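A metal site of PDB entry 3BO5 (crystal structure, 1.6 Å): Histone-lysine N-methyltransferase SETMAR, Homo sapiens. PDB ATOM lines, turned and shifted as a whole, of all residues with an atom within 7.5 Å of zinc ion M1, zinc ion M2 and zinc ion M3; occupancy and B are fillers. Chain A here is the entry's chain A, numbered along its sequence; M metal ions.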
ATOM      1  N   PRO A  60      26.328 -17.509   2.194  1.00  0.00           N
ATOM      2  CA  PRO A  60      25.562 -16.518   2.967  1.00  0.00           C
ATOM      3  C   PRO A  60      24.045 -16.683   2.954  1.00  0.00           C
ATOM      4  O   PRO A  60      23.362 -16.045   3.770  1.00  0.00           O
ATOM      5  CB  PRO A  60      25.884 -15.202   2.309  1.00  0.00           C
ATOM      6  CG  PRO A  60      26.393 -15.491   0.974  1.00  0.00           C
ATOM      7  CD  PRO A  60      26.999 -16.920   1.015  1.00  0.00           C
ATOM      8  N   GLY A  61      23.613 -17.552   2.075  1.00  0.00           N
ATOM      9  CA  GLY A  61      22.162 -17.888   2.020  1.00  0.00           C
ATOM     10  C   GLY A  61      21.361 -17.006   1.074  1.00  0.00           C
ATOM     11  O   GLY A  61      21.892 -16.114   0.367  1.00  0.00           O
ATOM     12  N   CYS A  62      20.037 -17.248   1.072  1.00  0.00           N
ATOM     13  CA  CYS A  62      19.167 -16.454   0.210  1.00  0.00           C
ATOM     14  C   CYS A  62      18.576 -15.317   1.001  1.00  0.00           C
ATOM     15  O   CYS A  62      18.670 -15.225   2.237  1.00  0.00           O
ATOM     16  CB  CYS A  62      18.063 -17.350  -0.315  1.00  0.00           C
ATOM     17  SG  CYS A  62      16.996 -18.050   0.980  1.00  0.00           S
ATOM     18  N   ILE A  63      17.903 -14.430   0.215  1.00  0.00           N
ATOM     19  CA  ILE A  63      17.364 -13.245   0.865  1.00  0.00           C
ATOM     20  C   ILE A  63      15.875 -13.319   1.142  1.00  0.00           C
ATOM     21  O   ILE A  63      15.297 -12.340   1.592  1.00  0.00           O
ATOM     22  CB  ILE A  63      17.620 -11.959   0.037  1.00  0.00           C
ATOM     23  CG1 ILE A  63      16.877 -11.989  -1.292  1.00  0.00           C
ATOM     24  CG2 ILE A  63      19.151 -11.757  -0.150  1.00  0.00           C
ATOM     25  CD1 ILE A  63      16.990 -10.657  -2.121  1.00  0.00           C
ATOM     26  N   CYS A  64      15.295 -14.488   0.976  1.00  0.00           N
ATOM     27  CA  CYS A  64      13.847 -14.613   1.075  1.00  0.00           C
ATOM     28  C   CYS A  64      13.485 -14.505   2.520  1.00  0.00           C
ATOM     29  O   CYS A  64      14.140 -15.125   3.385  1.00  0.00           O
ATOM     30  CB  CYS A  64      13.463 -16.007   0.614  1.00  0.00           C
ATOM     31  SG  CYS A  64      14.210 -16.412  -0.961  1.00  0.00           S
ATOM     32  N   VAL A  65      12.542 -13.623   2.816  1.00  0.00           N
ATOM     33  CA  VAL A  65      12.014 -13.628   4.187  1.00  0.00           C
ATOM     34  C   VAL A  65      10.529 -13.370   4.171  1.00  0.00           C
ATOM     35  O   VAL A  65       9.789 -14.016   4.932  1.00  0.00           O
ATOM     36  CB  VAL A  65      12.711 -12.623   5.097  1.00  0.00           C
ATOM     37  CG1 VAL A  65      12.581 -11.176   4.544  1.00  0.00           C
ATOM     38  CG2 VAL A  65      12.177 -12.846   6.600  1.00  0.00           C
ATOM     39  N   THR A  67       8.321 -14.073   1.699  1.00  0.00           N
ATOM     40  CA  THR A  67       7.497 -15.105   1.026  1.00  0.00           C
ATOM     41  C   THR A  67       8.358 -16.339   0.906  1.00  0.00           C
ATOM     42  O   THR A  67       9.578 -16.227   1.059  1.00  0.00           O
ATOM     43  CB  THR A  67       7.049 -14.670  -0.428  1.00  0.00           C
ATOM     44  OG1 THR A  67       8.216 -14.386  -1.208  1.00  0.00           O
ATOM     45  CG2 THR A  67       6.189 -13.406  -0.359  1.00  0.00           C
ATOM     46  N   PRO A  68       7.744 -17.494   0.637  1.00  0.00           N
ATOM     47  CA  PRO A  68       8.548 -18.716   0.574  1.00  0.00           C
ATOM     48  C   PRO A  68       9.620 -18.683  -0.517  1.00  0.00           C
ATOM     49  O   PRO A  68       9.558 -17.966  -1.527  1.00  0.00           O
ATOM     50  CB  PRO A  68       7.518 -19.808   0.235  1.00  0.00           C
ATOM     51  CG  PRO A  68       6.211 -19.247   0.901  1.00  0.00           C
ATOM     52  CD  PRO A  68       6.285 -17.774   0.578  1.00  0.00           C
ATOM     53  N   CYS A  69      10.606 -19.555  -0.291  1.00  0.00           N
ATOM     54  CA  CYS A  69      11.640 -19.705  -1.223  1.00  0.00           C
ATOM     55  C   CYS A  69      11.072 -20.422  -2.458  1.00  0.00           C
ATOM     56  O   CYS A  69      10.598 -21.572  -2.385  1.00  0.00           O
ATOM     57  CB  CYS A  69      12.761 -20.553  -0.584  1.00  0.00           C
ATOM     58  SG  CYS A  69      13.510 -19.666   0.764  1.00  0.00           S
ATOM     59  N   LEU A  70      11.198 -19.737  -3.554  1.00  0.00           N
ATOM     60  CA  LEU A  70      10.760 -20.319  -4.843  1.00  0.00           C
ATOM     61  C   LEU A  70      11.759 -20.019  -5.939  1.00  0.00           C
ATOM     62  O   LEU A  70      12.502 -19.005  -5.911  1.00  0.00           O
ATOM     63  CB  LEU A  70       9.358 -19.825  -5.195  1.00  0.00           C
ATOM     64  CG  LEU A  70       8.215 -20.369  -4.317  1.00  0.00           C
ATOM     65  CD1 LEU A  70       7.029 -19.409  -4.473  1.00  0.00           C
ATOM     66  CD2 LEU A  70       7.838 -21.770  -4.678  1.00  0.00           C
ATOM     67  N   THR A  73      13.332 -16.417  -7.437  1.00  0.00           N
ATOM     68  CA  THR A  73      13.510 -15.353  -6.437  1.00  0.00           C
ATOM     69  C   THR A  73      14.431 -15.820  -5.283  1.00  0.00           C
ATOM     70  O   THR A  73      14.913 -15.031  -4.489  1.00  0.00           O
ATOM     71  CB  THR A  73      12.181 -14.832  -5.905  1.00  0.00           C
ATOM     72  OG1 THR A  73      11.402 -15.918  -5.411  1.00  0.00           O
ATOM     73  CG2 THR A  73      11.351 -14.235  -7.055  1.00  0.00           C
ATOM     74  N   CYS A  74      14.696 -17.114  -5.238  1.00  0.00           N
ATOM     75  CA  CYS A  74      15.504 -17.687  -4.160  1.00  0.00           C
ATOM     76  C   CYS A  74      16.836 -18.089  -4.707  1.00  0.00           C
ATOM     77  O   CYS A  74      16.909 -18.926  -5.626  1.00  0.00           O
ATOM     78  CB  CYS A  74      14.806 -18.913  -3.593  1.00  0.00           C
ATOM     79  SG  CYS A  74      15.852 -19.663  -2.315  1.00  0.00           S
ATOM     80  N   SER A  75      17.890 -17.435  -4.217  1.00  0.00           N
ATOM     81  CA  SER A  75      19.249 -17.748  -4.749  1.00  0.00           C
ATOM     82  C   SER A  75      19.735 -19.131  -4.372  1.00  0.00           C
ATOM     83  O   SER A  75      20.711 -19.652  -4.910  1.00  0.00           O
ATOM     84  CB  SER A  75      20.293 -16.690  -4.357  1.00  0.00           C
ATOM     85  OG  SER A  75      20.326 -16.464  -2.958  1.00  0.00           O
ATOM     86  N   CYS A  76      19.048 -19.757  -3.426  1.00  0.00           N
ATOM     87  CA  CYS A  76      19.301 -21.177  -3.139  1.00  0.00           C
ATOM     88  C   CYS A  76      18.666 -22.154  -4.137  1.00  0.00           C
ATOM     89  O   CYS A  76      18.978 -23.362  -4.062  1.00  0.00           O
ATOM     90  CB  CYS A  76      18.833 -21.556  -1.712  1.00  0.00           C
ATOM     91  SG  CYS A  76      19.636 -20.623  -0.458  1.00  0.00           S
ATOM     92  N   LEU A  77      17.775 -21.677  -4.999  1.00  0.00           N
ATOM     93  CA  LEU A  77      17.013 -22.502  -5.907  1.00  0.00           C
ATOM     94  C   LEU A  77      17.277 -22.116  -7.341  1.00  0.00           C
ATOM     95  O   LEU A  77      16.331 -22.032  -8.137  1.00  0.00           O
ATOM     96  CB  LEU A  77      15.516 -22.357  -5.652  1.00  0.00           C
ATOM     97  CG  LEU A  77      15.086 -22.922  -4.308  1.00  0.00           C
ATOM     98  CD1 LEU A  77      13.560 -22.821  -4.089  1.00  0.00           C
ATOM     99  CD2 LEU A  77      15.508 -24.349  -4.148  1.00  0.00           C
ATOM    100  N   PHE A 103      21.711 -26.985  -3.535  1.00  0.00           N
ATOM    101  CA  PHE A 103      21.936 -26.205  -2.318  1.00  0.00           C
ATOM    102  C   PHE A 103      20.661 -26.183  -1.523  1.00  0.00           C
ATOM    103  O   PHE A 103      19.645 -25.859  -2.062  1.00  0.00           O
ATOM    104  CB  PHE A 103      22.318 -24.767  -2.696  1.00  0.00           C
ATOM    105  CG  PHE A 103      23.673 -24.682  -3.274  1.00  0.00           C
ATOM    106  CD1 PHE A 103      24.767 -24.369  -2.454  1.00  0.00           C
ATOM    107  CD2 PHE A 103      23.859 -24.902  -4.652  1.00  0.00           C
ATOM    108  CE1 PHE A 103      26.068 -24.301  -2.988  1.00  0.00           C
ATOM    109  CE2 PHE A 103      25.171 -24.823  -5.201  1.00  0.00           C
ATOM    110  CZ  PHE A 103      26.225 -24.523  -4.376  1.00  0.00           C
ATOM    111  N   GLU A 104      20.727 -26.571  -0.263  1.00  0.00           N
ATOM    112  CA  GLU A 104      19.599 -26.324   0.679  1.00  0.00           C
ATOM    113  C   GLU A 104      19.694 -24.923   1.285  1.00  0.00           C
ATOM    114  O   GLU A 104      20.792 -24.345   1.408  1.00  0.00           O
ATOM    115  CB  GLU A 104      19.582 -27.369   1.821  1.00  0.00           C
ATOM    116  CG  GLU A 104      19.237 -28.719   1.258  1.00  0.00           C
ATOM    117  CD  GLU A 104      18.749 -29.724   2.321  1.00  0.00           C
ATOM    118  OE1 GLU A 104      18.721 -29.417   3.558  1.00  0.00           O
ATOM    119  OE2 GLU A 104      18.480 -30.847   1.835  1.00  0.00           O
ATOM    120  N   CYS A 105      18.533 -24.410   1.753  1.00  0.00           N
ATOM    121  CA  CYS A 105      18.589 -23.216   2.591  1.00  0.00           C
ATOM    122  C   CYS A 105      19.335 -23.605   3.882  1.00  0.00           C
ATOM    123  O   CYS A 105      19.362 -24.755   4.275  1.00  0.00           O
ATOM    124  CB  CYS A 105      17.197 -22.693   2.822  1.00  0.00           C
ATOM    125  SG  CYS A 105      16.560 -21.989   1.362  1.00  0.00           S
ATOM    126  N   ASN A 106      20.083 -22.622   4.424  1.00  0.00           N
ATOM    127  CA  ASN A 106      21.012 -22.901   5.480  1.00  0.00           C
ATOM    128  C   ASN A 106      20.783 -22.049   6.716  1.00  0.00           C
ATOM    129  O   ASN A 106      19.745 -21.450   6.863  1.00  0.00           O
ATOM    130  CB  ASN A 106      22.451 -22.852   4.977  1.00  0.00           C
ATOM    131  CG  ASN A 106      22.901 -21.452   4.617  1.00  0.00           C
ATOM    132  OD1 ASN A 106      22.357 -20.471   5.090  1.00  0.00           O
ATOM    133  ND2 ASN A 106      23.987 -21.354   3.820  1.00  0.00           N
ATOM    134  N   LEU A 108      21.872 -19.351   7.598  1.00  0.00           N
ATOM    135  CA  LEU A 108      21.805 -17.929   7.356  1.00  0.00           C
ATOM    136  C   LEU A 108      20.609 -17.468   6.547  1.00  0.00           C
ATOM    137  O   LEU A 108      20.344 -16.209   6.435  1.00  0.00           O
ATOM    138  CB  LEU A 108      23.074 -17.462   6.702  1.00  0.00           C
ATOM    139  CG  LEU A 108      24.283 -17.737   7.601  1.00  0.00           C
ATOM    140  CD1 LEU A 108      25.414 -17.109   6.797  1.00  0.00           C
ATOM    141  CD2 LEU A 108      24.169 -17.150   9.019  1.00  0.00           C
ATOM    142  N   CYS A 109      19.912 -18.397   5.888  1.00  0.00           N
ATOM    143  CA  CYS A 109      18.714 -18.063   5.135  1.00  0.00           C
ATOM    144  C   CYS A 109      17.652 -17.621   6.163  1.00  0.00           C
ATOM    145  O   CYS A 109      17.477 -18.296   7.147  1.00  0.00           O
ATOM    146  CB  CYS A 109      18.250 -19.311   4.332  1.00  0.00           C
ATOM    147  SG  CYS A 109      19.430 -19.765   3.051  1.00  0.00           S
ATOM    148  N   ARG A 110      16.874 -16.597   5.820  1.00  0.00           N
ATOM    149  CA  ARG A 110      15.891 -16.160   6.795  1.00  0.00           C
ATOM    150  C   ARG A 110      14.554 -16.777   6.570  1.00  0.00           C
ATOM    151  O   ARG A 110      13.654 -16.556   7.398  1.00  0.00           O
ATOM    152  CB  ARG A 110      15.783 -14.659   6.792  1.00  0.00           C
ATOM    153  CG  ARG A 110      17.004 -14.070   7.455  1.00  0.00           C
ATOM    154  CD  ARG A 110      17.428 -12.790   6.792  1.00  0.00           C
ATOM    155  NE  ARG A 110      16.443 -11.787   7.078  1.00  0.00           N
ATOM    156  CZ  ARG A 110      16.491 -10.541   6.637  1.00  0.00           C
ATOM    157  NH1 ARG A 110      15.506  -9.694   6.966  1.00  0.00           N
ATOM    158  NH2 ARG A 110      17.506 -10.147   5.877  1.00  0.00           N
ATOM    159  N   CYS A 111      14.424 -17.613   5.527  1.00  0.00           N
ATOM    160  CA  CYS A 111      13.221 -18.436   5.443  1.00  0.00           C
ATOM    161  C   CYS A 111      13.031 -19.297   6.693  1.00  0.00           C
ATOM    162  O   CYS A 111      14.006 -19.600   7.415  1.00  0.00           O
ATOM    163  CB  CYS A 111      13.231 -19.322   4.189  1.00  0.00           C
ATOM    164  SG  CYS A 111      14.747 -20.381   4.224  1.00  0.00           S
ATOM    165  N   SER A 112      11.812 -19.734   6.964  1.00  0.00           N
ATOM    166  CA  SER A 112      11.572 -20.485   8.185  1.00  0.00           C
ATOM    167  C   SER A 112      12.131 -21.867   8.117  1.00  0.00           C
ATOM    168  O   SER A 112      12.512 -22.368   7.019  1.00  0.00           O
ATOM    169  CB  SER A 112      10.094 -20.601   8.526  1.00  0.00           C
ATOM    170  OG  SER A 112       9.506 -21.606   7.738  1.00  0.00           O
ATOM    171  N   HIS A 114      10.542 -24.331   8.123  1.00  0.00           N
ATOM    172  CA  HIS A 114       9.563 -25.067   7.299  1.00  0.00           C
ATOM    173  C   HIS A 114       9.779 -24.967   5.806  1.00  0.00           C
ATOM    174  O   HIS A 114       9.030 -25.516   4.976  1.00  0.00           O
ATOM    175  CB  HIS A 114       8.155 -24.692   7.705  1.00  0.00           C
ATOM    176  CG  HIS A 114       7.928 -24.883   9.168  1.00  0.00           C
ATOM    177  ND1 HIS A 114       7.787 -23.837  10.055  1.00  0.00           N
ATOM    178  CD2 HIS A 114       7.949 -26.012   9.924  1.00  0.00           C
ATOM    179  CE1 HIS A 114       7.661 -24.303  11.282  1.00  0.00           C
ATOM    180  NE2 HIS A 114       7.761 -25.629  11.236  1.00  0.00           N
ATOM    181  N   CYS A 115      10.820 -24.233   5.433  1.00  0.00           N
ATOM    182  CA  CYS A 115      11.070 -24.029   4.045  1.00  0.00           C
ATOM    183  C   CYS A 115      11.208 -25.413   3.381  1.00  0.00           C
ATOM    184  O   CYS A 115      11.887 -26.293   3.912  1.00  0.00           O
ATOM    185  CB  CYS A 115      12.412 -23.279   3.882  1.00  0.00           C
ATOM    186  SG  CYS A 115      12.947 -23.080   2.161  1.00  0.00           S
ATOM    187  N   ARG A 116      10.591 -25.564   2.204  1.00  0.00           N
ATOM    188  CA  ARG A 116      10.659 -26.834   1.450  1.00  0.00           C
ATOM    189  C   ARG A 116      12.049 -27.175   0.962  1.00  0.00           C
ATOM    190  O   ARG A 116      12.255 -28.345   0.579  1.00  0.00           O
ATOM    191  CB  ARG A 116       9.706 -26.869   0.253  1.00  0.00           C
ATOM    192  CG  ARG A 116       8.277 -27.063   0.801  1.00  0.00           C
ATOM    193  CD  ARG A 116       7.240 -26.479  -0.146  1.00  0.00           C
ATOM    194  NE  ARG A 116       7.093 -27.183  -1.417  1.00  0.00           N
ATOM    195  CZ  ARG A 116       6.148 -26.875  -2.304  1.00  0.00           C
ATOM    196  NH1 ARG A 116       6.049 -27.545  -3.437  1.00  0.00           N
ATOM    197  NH2 ARG A 116       5.296 -25.885  -2.040  1.00  0.00           N
ATOM    198  N   ASN A 117      12.958 -26.201   0.994  1.00  0.00           N
ATOM    199  CA  ASN A 117      14.332 -26.483   0.578  1.00  0.00           C
ATOM    200  C   ASN A 117      15.241 -26.770   1.771  1.00  0.00           C
ATOM    201  O   ASN A 117      16.457 -26.551   1.661  1.00  0.00           O
ATOM    202  CB  ASN A 117      14.898 -25.326  -0.288  1.00  0.00           C
ATOM    203  CG  ASN A 117      16.106 -25.716  -1.046  1.00  0.00           C
ATOM    204  OD1 ASN A 117      16.121 -26.776  -1.667  1.00  0.00           O
ATOM    205  ND2 ASN A 117      17.094 -24.821  -1.089  1.00  0.00           N
ATOM    206  N   ARG A 118      14.653 -27.274   2.868  1.00  0.00           N
ATOM    207  CA  ARG A 118      15.433 -27.797   4.032  1.00  0.00           C
ATOM    208  C   ARG A 118      14.965 -29.221   4.206  1.00  0.00           C
ATOM    209  O   ARG A 118      13.805 -29.444   4.605  1.00  0.00           O
ATOM    210  CB  ARG A 118      15.139 -26.980   5.304  1.00  0.00           C
ATOM    211  CG  ARG A 118      15.444 -25.502   5.138  1.00  0.00           C
ATOM    212  CD  ARG A 118      14.977 -24.785   6.354  1.00  0.00           C
ATOM    213  NE  ARG A 118      15.260 -23.331   6.359  1.00  0.00           N
ATOM    214  CZ  ARG A 118      16.398 -22.776   6.704  1.00  0.00           C
ATOM    215  NH1 ARG A 118      17.476 -23.511   6.940  1.00  0.00           N
ATOM    216  NH2 ARG A 118      16.470 -21.414   6.742  1.00  0.00           N
HETATM  217 ZN    ZN M   1      15.195 -18.476  -0.490  1.00  0.00          ZN
HETATM  218 ZN    ZN M   2      18.062 -20.181   1.161  1.00  0.00          ZN
HETATM  219 ZN    ZN M   3      14.429 -21.333   2.158  1.00  0.00          ZN
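The side-chain sulfur (SG) of Cys 74 sits close to the backbone NH (N) of Cys 76 (3.4 Å).
The side-chain sulfur of Cys 115 lies close to the backbone NH of Asn 117 (3.3 Å).
The backbone carbonyl oxygen (O) of Cys 64 lies within hydrogen-bond range of the backbone NH (N) of Cys 111 (3.3 Å).
The guanidinium group of Arg 118 is in hydrogen-bond range of the backbone carbonyl oxygen of Cys 111 (3.1 Å).
O of Asn 117 is in hydrogen-bond range of N of Cys 105.
O of Cys 105 is in hydrogen-bond range of NH1 of Arg 118 (3.5 Å).
The backbone NH of Cys 109 sits at hydrogen-bond distance from the side-chain amide oxygen of Asn 106 (3.3 Å).
NH2 of Arg 118 lies within hydrogen-bond range of O of Cys 109 (3.3 Å).
The nearest printed residue that does not touch zinc ion M1 is Cys 105 (4.2 Å).
Of the 29 residues printed, 4 come within 4 Å of zinc ion M2.
The nearest printed residue that does not touch zinc ion M2 is Cys 74 (4.2 Å).
Four residues have an atom within 4 Å of zinc ion M3: Cys 69, Cys 105, Cys 111 and Cys 115.
The nearest printed residue that does not touch zinc ion M3 is Cys 62 (4.3 Å).
The side-chain sulfur (SG) of Cys 74 is bound to zinc ion M1 (2.3 Å).
The side-chain sulfur (SG) of Cys 64 binds zinc ion M1 (2.3 Å).
SG of Cys 62 is bound to zinc ion M1 (2.4 Å).
SG of Cys 69 is bound to zinc ion M1 (2.4 Å).
SG of Cys 76 binds zinc ion M2 (2.3 Å).
Zinc ion M2 is bound by SG of Cys 105 (2.4 Å).
The side-chain sulfur (SG) of Cys 109 is bound to zinc ion M2 (2.4 Å).
SG of Cys 62 binds zinc ion M2 (2.4 Å).
Zinc ion M2 has four donor atoms within binding distance.
Zinc ion M3 is bound by SG of Cys 115 (2.3 Å), SG of Cys 111 (2.3 Å), SG of Cys 69 (2.4 Å) and SG of Cys 105 (2.4 Å).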
